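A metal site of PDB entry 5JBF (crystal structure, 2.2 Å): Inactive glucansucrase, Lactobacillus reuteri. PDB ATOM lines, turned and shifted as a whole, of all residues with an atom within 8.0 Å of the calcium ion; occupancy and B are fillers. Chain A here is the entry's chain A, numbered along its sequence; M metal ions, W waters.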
ATOM      1  N   LEU A 190      17.516  34.508  16.980  1.00  0.00           N
ATOM      2  CA  LEU A 190      18.561  33.829  17.733  1.00  0.00           C
ATOM      3  C   LEU A 190      19.411  33.029  16.714  1.00  0.00           C
ATOM      4  O   LEU A 190      18.978  31.984  16.211  1.00  0.00           O
ATOM      5  CB  LEU A 190      17.979  32.900  18.807  1.00  0.00           C
ATOM      6  CG  LEU A 190      17.006  33.506  19.838  1.00  0.00           C
ATOM      7  CD1 LEU A 190      16.695  32.443  20.886  1.00  0.00           C
ATOM      8  CD2 LEU A 190      17.563  34.759  20.504  1.00  0.00           C
ATOM      9  N   MET A 191      20.599  33.535  16.416  1.00  0.00           N
ATOM     10  CA  MET A 191      21.470  32.952  15.405  1.00  0.00           C
ATOM     11  C   MET A 191      22.490  32.001  16.025  1.00  0.00           C
ATOM     12  O   MET A 191      22.927  32.195  17.146  1.00  0.00           O
ATOM     13  CB  MET A 191      22.179  34.063  14.638  1.00  0.00           C
ATOM     14  CG  MET A 191      21.247  34.840  13.716  1.00  0.00           C
ATOM     15  SD  MET A 191      22.179  36.018  12.732  1.00  0.00           S
ATOM     16  CE  MET A 191      23.044  34.983  11.558  1.00  0.00           C
ATOM     17  N   ASN A 192      22.809  30.947  15.275  1.00  0.00           N
ATOM     18  CA  ASN A 192      23.831  29.982  15.660  1.00  0.00           C
ATOM     19  C   ASN A 192      23.457  29.165  16.883  1.00  0.00           C
ATOM     20  O   ASN A 192      24.324  28.727  17.623  1.00  0.00           O
ATOM     21  CB  ASN A 192      25.205  30.674  15.876  1.00  0.00           C
ATOM     22  CG  ASN A 192      25.553  31.630  14.752  1.00  0.00           C
ATOM     23  OD1 ASN A 192      25.747  31.247  13.620  1.00  0.00           O
ATOM     24  ND2 ASN A 192      25.679  32.859  15.079  1.00  0.00           N
ATOM     25  N   THR A 194      22.845  26.219  17.011  1.00  0.00           N
ATOM     26  CA  THR A 194      23.063  25.082  16.125  1.00  0.00           C
ATOM     27  C   THR A 194      23.783  23.978  16.872  1.00  0.00           C
ATOM     28  O   THR A 194      24.719  24.235  17.651  1.00  0.00           O
ATOM     29  CB  THR A 194      23.906  25.497  14.913  1.00  0.00           C
ATOM     30  OG1 THR A 194      25.075  26.248  15.353  1.00  0.00           O
ATOM     31  CG2 THR A 194      23.058  26.371  13.950  1.00  0.00           C
ATOM     32  N   PRO A 208      27.779  27.298  11.647  1.00  0.00           N
ATOM     33  CA  PRO A 208      27.255  28.608  11.212  1.00  0.00           C
ATOM     34  C   PRO A 208      25.767  28.645  10.894  1.00  0.00           C
ATOM     35  O   PRO A 208      25.224  27.701  10.329  1.00  0.00           O
ATOM     36  CB  PRO A 208      28.032  28.866   9.911  1.00  0.00           C
ATOM     37  CG  PRO A 208      28.261  27.504   9.361  1.00  0.00           C
ATOM     38  CD  PRO A 208      28.561  26.647  10.575  1.00  0.00           C
ATOM     39  N   GLU A 209      25.141  29.788  11.211  1.00  0.00           N
ATOM     40  CA  GLU A 209      23.742  30.004  10.905  1.00  0.00           C
ATOM     41  C   GLU A 209      23.536  30.140   9.400  1.00  0.00           C
ATOM     42  O   GLU A 209      22.574  29.629   8.856  1.00  0.00           O
ATOM     43  CB  GLU A 209      23.216  31.244  11.634  1.00  0.00           C
ATOM     44  CG  GLU A 209      21.732  31.538  11.413  1.00  0.00           C
ATOM     45  CD  GLU A 209      20.807  30.402  11.857  1.00  0.00           C
ATOM     46  OE1 GLU A 209      20.871  30.072  13.082  1.00  0.00           O
ATOM     47  OE2 GLU A 209      20.053  29.841  10.978  1.00  0.00           O
ATOM     48  N   LEU A 210      24.453  30.803   8.730  1.00  0.00           N
ATOM     49  CA  LEU A 210      24.219  31.211   7.358  1.00  0.00           C
ATOM     50  C   LEU A 210      24.983  30.365   6.391  1.00  0.00           C
ATOM     51  O   LEU A 210      26.145  30.093   6.594  1.00  0.00           O
ATOM     52  CB  LEU A 210      24.606  32.671   7.193  1.00  0.00           C
ATOM     53  CG  LEU A 210      23.942  33.647   8.164  1.00  0.00           C
ATOM     54  CD1 LEU A 210      24.510  35.058   7.976  1.00  0.00           C
ATOM     55  CD2 LEU A 210      22.426  33.631   7.971  1.00  0.00           C
ATOM     56  N   LEU A 211      24.314  29.988   5.298  1.00  0.00           N
ATOM     57  CA  LEU A 211      24.902  29.250   4.193  1.00  0.00           C
ATOM     58  C   LEU A 211      24.735  30.069   2.925  1.00  0.00           C
ATOM     59  O   LEU A 211      25.709  30.654   2.440  1.00  0.00           O
ATOM     60  CB  LEU A 211      24.234  27.885   4.033  1.00  0.00           C
ATOM     61  CG  LEU A 211      24.452  26.827   5.082  1.00  0.00           C
ATOM     62  CD1 LEU A 211      23.708  25.583   4.601  1.00  0.00           C
ATOM     63  CD2 LEU A 211      25.926  26.470   5.310  1.00  0.00           C
ATOM     64  N   VAL A 212      23.528  30.123   2.401  1.00  0.00           N
ATOM     65  CA  VAL A 212      23.289  30.807   1.145  1.00  0.00           C
ATOM     66  C   VAL A 212      21.790  31.101   1.044  1.00  0.00           C
ATOM     67  O   VAL A 212      20.966  30.351   1.548  1.00  0.00           O
ATOM     68  CB  VAL A 212      23.775  29.998  -0.055  1.00  0.00           C
ATOM     69  CG1 VAL A 212      22.920  28.740  -0.253  1.00  0.00           C
ATOM     70  CG2 VAL A 212      23.797  30.821  -1.333  1.00  0.00           C
ATOM     71  N   ASN A 214      18.166  33.607   1.297  1.00  0.00           N
ATOM     72  CA  ASN A 214      17.456  34.221   2.404  1.00  0.00           C
ATOM     73  C   ASN A 214      17.359  33.199   3.530  1.00  0.00           C
ATOM     74  O   ASN A 214      16.568  32.229   3.453  1.00  0.00           O
ATOM     75  CB  ASN A 214      16.056  34.679   1.990  1.00  0.00           C
ATOM     76  CG  ASN A 214      16.098  35.827   1.008  1.00  0.00           C
ATOM     77  OD1 ASN A 214      16.466  35.637  -0.134  1.00  0.00           O
ATOM     78  ND2 ASN A 214      15.688  37.021   1.434  1.00  0.00           N
ATOM     79  N   ASP A 215      18.131  33.442   4.600  1.00  0.00           N
ATOM     80  CA  ASP A 215      18.170  32.546   5.757  1.00  0.00           C
ATOM     81  C   ASP A 215      16.940  32.736   6.653  1.00  0.00           C
ATOM     82  O   ASP A 215      16.648  33.881   7.104  1.00  0.00           O
ATOM     83  CB  ASP A 215      19.441  32.774   6.557  1.00  0.00           C
ATOM     84  CG  ASP A 215      19.723  31.665   7.547  1.00  0.00           C
ATOM     85  OD1 ASP A 215      20.199  30.564   7.116  1.00  0.00           O
ATOM     86  OD2 ASP A 215      19.458  31.854   8.742  1.00  0.00           O
ATOM     87  N   ILE A 216      16.217  31.653   6.886  1.00  0.00           N
ATOM     88  CA  ILE A 216      14.948  31.700   7.606  1.00  0.00           C
ATOM     89  C   ILE A 216      15.209  31.716   9.115  1.00  0.00           C
ATOM     90  O   ILE A 216      16.045  30.953   9.607  1.00  0.00           O
ATOM     91  CB  ILE A 216      14.067  30.464   7.219  1.00  0.00           C
ATOM     92  CG1 ILE A 216      13.731  30.445   5.725  1.00  0.00           C
ATOM     93  CG2 ILE A 216      12.802  30.403   8.061  1.00  0.00           C
ATOM     94  CD1 ILE A 216      12.924  31.650   5.247  1.00  0.00           C
ATOM     95  N   ASP A 217      14.438  32.536   9.846  1.00  0.00           N
ATOM     96  CA  ASP A 217      14.554  32.606  11.304  1.00  0.00           C
ATOM     97  C   ASP A 217      13.794  31.443  11.967  1.00  0.00           C
ATOM     98  O   ASP A 217      12.690  31.587  12.469  1.00  0.00           O
ATOM     99  CB  ASP A 217      14.134  33.964  11.875  1.00  0.00           C
ATOM    100  CG  ASP A 217      14.383  34.069  13.362  1.00  0.00           C
ATOM    101  OD1 ASP A 217      15.067  33.178  13.942  1.00  0.00           O
ATOM    102  OD2 ASP A 217      13.913  35.052  13.956  1.00  0.00           O
ATOM    103  N   ASN A 218      14.463  30.296  12.027  1.00  0.00           N
ATOM    104  CA  ASN A 218      13.949  29.127  12.712  1.00  0.00           C
ATOM    105  C   ASN A 218      13.931  29.225  14.235  1.00  0.00           C
ATOM    106  O   ASN A 218      13.522  28.239  14.905  1.00  0.00           O
ATOM    107  CB  ASN A 218      14.684  27.859  12.242  1.00  0.00           C
ATOM    108  CG  ASN A 218      14.382  27.552  10.790  1.00  0.00           C
ATOM    109  OD1 ASN A 218      13.254  27.197  10.449  1.00  0.00           O
ATOM    110  ND2 ASN A 218      15.374  27.726   9.912  1.00  0.00           N
ATOM    111  N   ALA A 256      20.598  20.842   5.887  1.00  0.00           N
ATOM    112  CA  ALA A 256      21.244  21.891   6.701  1.00  0.00           C
ATOM    113  C   ALA A 256      20.895  21.806   8.179  1.00  0.00           C
ATOM    114  O   ALA A 256      20.740  22.838   8.862  1.00  0.00           O
ATOM    115  CB  ALA A 256      20.900  23.271   6.142  1.00  0.00           C
ATOM    116  N   ASP A 258      22.722  21.190  10.585  1.00  0.00           N
ATOM    117  CA  ASP A 258      23.724  21.937  11.357  1.00  0.00           C
ATOM    118  C   ASP A 258      23.599  23.489  11.319  1.00  0.00           C
ATOM    119  O   ASP A 258      24.300  24.191  12.036  1.00  0.00           O
ATOM    120  CB  ASP A 258      25.121  21.592  10.832  1.00  0.00           C
ATOM    121  CG  ASP A 258      25.501  20.079  11.007  1.00  0.00           C
ATOM    122  OD1 ASP A 258      24.743  19.344  11.720  1.00  0.00           O
ATOM    123  OD2 ASP A 258      26.553  19.690  10.427  1.00  0.00           O
ATOM    124  N   ASN A 259      22.725  24.025  10.477  1.00  0.00           N
ATOM    125  CA  ASN A 259      22.670  25.474  10.207  1.00  0.00           C
ATOM    126  C   ASN A 259      21.284  26.090  10.454  1.00  0.00           C
ATOM    127  O   ASN A 259      20.994  27.156   9.962  1.00  0.00           O
ATOM    128  CB  ASN A 259      23.059  25.740   8.772  1.00  0.00           C
ATOM    129  CG  ASN A 259      24.249  24.932   8.347  1.00  0.00           C
ATOM    130  OD1 ASN A 259      24.089  23.954   7.628  1.00  0.00           O
ATOM    131  ND2 ASN A 259      25.436  25.300   8.793  1.00  0.00           N
ATOM    132  N   ILE A 260      20.476  25.419  11.249  1.00  0.00           N
ATOM    133  CA  ILE A 260      19.160  25.909  11.661  1.00  0.00           C
ATOM    134  C   ILE A 260      19.089  25.722  13.146  1.00  0.00           C
ATOM    135  O   ILE A 260      19.675  24.742  13.683  1.00  0.00           O
ATOM    136  CB  ILE A 260      18.038  25.101  10.965  1.00  0.00           C
ATOM    137  CG1 ILE A 260      18.134  23.590  11.293  1.00  0.00           C
ATOM    138  CG2 ILE A 260      18.094  25.367   9.478  1.00  0.00           C
ATOM    139  CD1 ILE A 260      17.271  22.673  10.405  1.00  0.00           C
ATOM    140  N   ASP A 261      18.373  26.611  13.808  1.00  0.00           N
ATOM    141  CA  ASP A 261      18.043  26.467  15.248  1.00  0.00           C
ATOM    142  C   ASP A 261      17.617  25.013  15.537  1.00  0.00           C
ATOM    143  O   ASP A 261      16.645  24.508  14.940  1.00  0.00           O
ATOM    144  CB  ASP A 261      16.912  27.458  15.628  1.00  0.00           C
ATOM    145  CG  ASP A 261      16.726  27.596  17.125  1.00  0.00           C
ATOM    146  OD1 ASP A 261      16.815  26.580  17.871  1.00  0.00           O
ATOM    147  OD2 ASP A 261      16.453  28.725  17.600  1.00  0.00           O
ATOM    148  N   MET A 722      14.466  23.724   5.629  1.00  0.00           N
ATOM    149  CA  MET A 722      14.073  24.799   6.557  1.00  0.00           C
ATOM    150  C   MET A 722      15.021  25.980   6.590  1.00  0.00           C
ATOM    151  O   MET A 722      14.684  27.027   7.141  1.00  0.00           O
ATOM    152  CB  MET A 722      13.908  24.238   7.984  1.00  0.00           C
ATOM    153  CG  MET A 722      12.658  23.352   8.128  1.00  0.00           C
ATOM    154  SD  MET A 722      12.384  22.684   9.764  1.00  0.00           S
ATOM    155  CE  MET A 722      13.398  21.200   9.677  1.00  0.00           C
ATOM    156  N   ASN A 723      16.219  25.811   6.015  1.00  0.00           N
ATOM    157  CA  ASN A 723      17.283  26.802   6.202  1.00  0.00           C
ATOM    158  C   ASN A 723      17.053  28.108   5.472  1.00  0.00           C
ATOM    159  O   ASN A 723      17.301  29.171   6.047  1.00  0.00           O
ATOM    160  CB  ASN A 723      18.611  26.282   5.710  1.00  0.00           C
ATOM    161  CG  ASN A 723      19.741  27.306   5.952  1.00  0.00           C
ATOM    162  OD1 ASN A 723      20.023  27.624   7.103  1.00  0.00           O
ATOM    163  ND2 ASN A 723      20.283  27.872   4.892  1.00  0.00           N
ATOM    164  N   GLN A 724      16.706  27.999   4.198  1.00  0.00           N
ATOM    165  CA  GLN A 724      16.625  29.167   3.334  1.00  0.00           C
ATOM    166  C   GLN A 724      15.547  29.051   2.272  1.00  0.00           C
ATOM    167  O   GLN A 724      15.074  27.942   1.954  1.00  0.00           O
ATOM    168  CB  GLN A 724      17.971  29.409   2.636  1.00  0.00           C
ATOM    169  CG  GLN A 724      18.240  28.649   1.338  1.00  0.00           C
ATOM    170  CD  GLN A 724      18.616  27.197   1.524  1.00  0.00           C
ATOM    171  OE1 GLN A 724      19.272  26.837   2.497  1.00  0.00           O
ATOM    172  NE2 GLN A 724      18.208  26.362   0.581  1.00  0.00           N
ATOM    173  N   ASN A 741      29.413  34.217   8.113  1.00  0.00           N
ATOM    174  CA  ASN A 741      28.350  33.211   8.172  1.00  0.00           C
ATOM    175  C   ASN A 741      27.752  32.946   9.562  1.00  0.00           C
ATOM    176  O   ASN A 741      26.797  32.194   9.670  1.00  0.00           O
ATOM    177  CB  ASN A 741      28.819  31.881   7.541  1.00  0.00           C
ATOM    178  CG  ASN A 741      29.929  31.224   8.308  1.00  0.00           C
ATOM    179  OD1 ASN A 741      30.423  31.771   9.295  1.00  0.00           O
ATOM    180  ND2 ASN A 741      30.369  30.085   7.839  1.00  0.00           N
ATOM    181  N   ASN A 814      16.644  35.842   9.115  1.00  0.00           N
ATOM    182  CA  ASN A 814      17.857  36.300   9.794  1.00  0.00           C
ATOM    183  C   ASN A 814      18.704  37.231   8.930  1.00  0.00           C
ATOM    184  O   ASN A 814      19.458  38.039   9.456  1.00  0.00           O
ATOM    185  CB  ASN A 814      18.776  35.103  10.183  1.00  0.00           C
ATOM    186  CG  ASN A 814      18.199  34.246  11.270  1.00  0.00           C
ATOM    187  OD1 ASN A 814      17.595  34.745  12.224  1.00  0.00           O
ATOM    188  ND2 ASN A 814      18.420  32.902  11.168  1.00  0.00           N
HETATM  189 CA    CA M   1      20.294  29.183   8.910  1.00  0.00          CA
HETATM  190  O   HOH W   1      17.837  29.128   8.729  1.00  0.00           O
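The backbone carbonyl oxygen of Asp 215 sits at hydrogen-bond distance from the backbone NH of Asn 814, at 2.8 Å.
The side-chain amide nitrogen of Asn 259 sits at hydrogen-bond distance from the backbone carbonyl oxygen of Pro 208, at 2.9 Å.
The side-chain amide oxygen (OD1) of Asn 192 sits at hydrogen-bond distance from the backbone NH (N) of Glu 209 (2.9 Å).
The side-chain amide nitrogen of Asn 814 lies close to the side-chain carboxylate of Glu 209, at 3.5 Å.
The side-chain amide nitrogen of Asn 723 sits at hydrogen-bond distance from the side-chain amide oxygen of Gln 724, 2.8 Å away.
The backbone carbonyl oxygen (O) of Asn 723 lies within hydrogen-bond range of the backbone NH (N) of Ile 216, 2.8 Å away.
O of Asn 741 sits at hydrogen-bond distance from N of Glu 209, at 3.3 Å.
Within 4 Å of the calcium ion: Glu 209, Asp 215, Asn 259 and Asn 723.
The nearest printed residue that does not touch the calcium ion is Ile 260 (4.4 Å).
The calcium ion is bound by the side-chain carboxylate (OE2) of Glu 209 (2.2 Å), the side-chain carboxylate (OD1) of Asp 215 (2.3 Å), the backbone carbonyl oxygen (O) of Glu 209 (2.3 Å), the backbone carbonyl oxygen (O) of Asn 259 (2.4 Å), the side-chain amide oxygen (OD1) of Asn 723 (2.4 Å), water W1 (2.5 Å) and the side-chain carboxylate (OD2) of Asp 215 (2.8 Å).
Water W1 lies within hydrogen-bond range of the backbone carbonyl oxygen of Ile 216 (2.7 Å), the backbone carbonyl oxygen of Asn 723 (2.7 Å) and the side-chain amide nitrogen of Asn 218 (3.1 Å).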
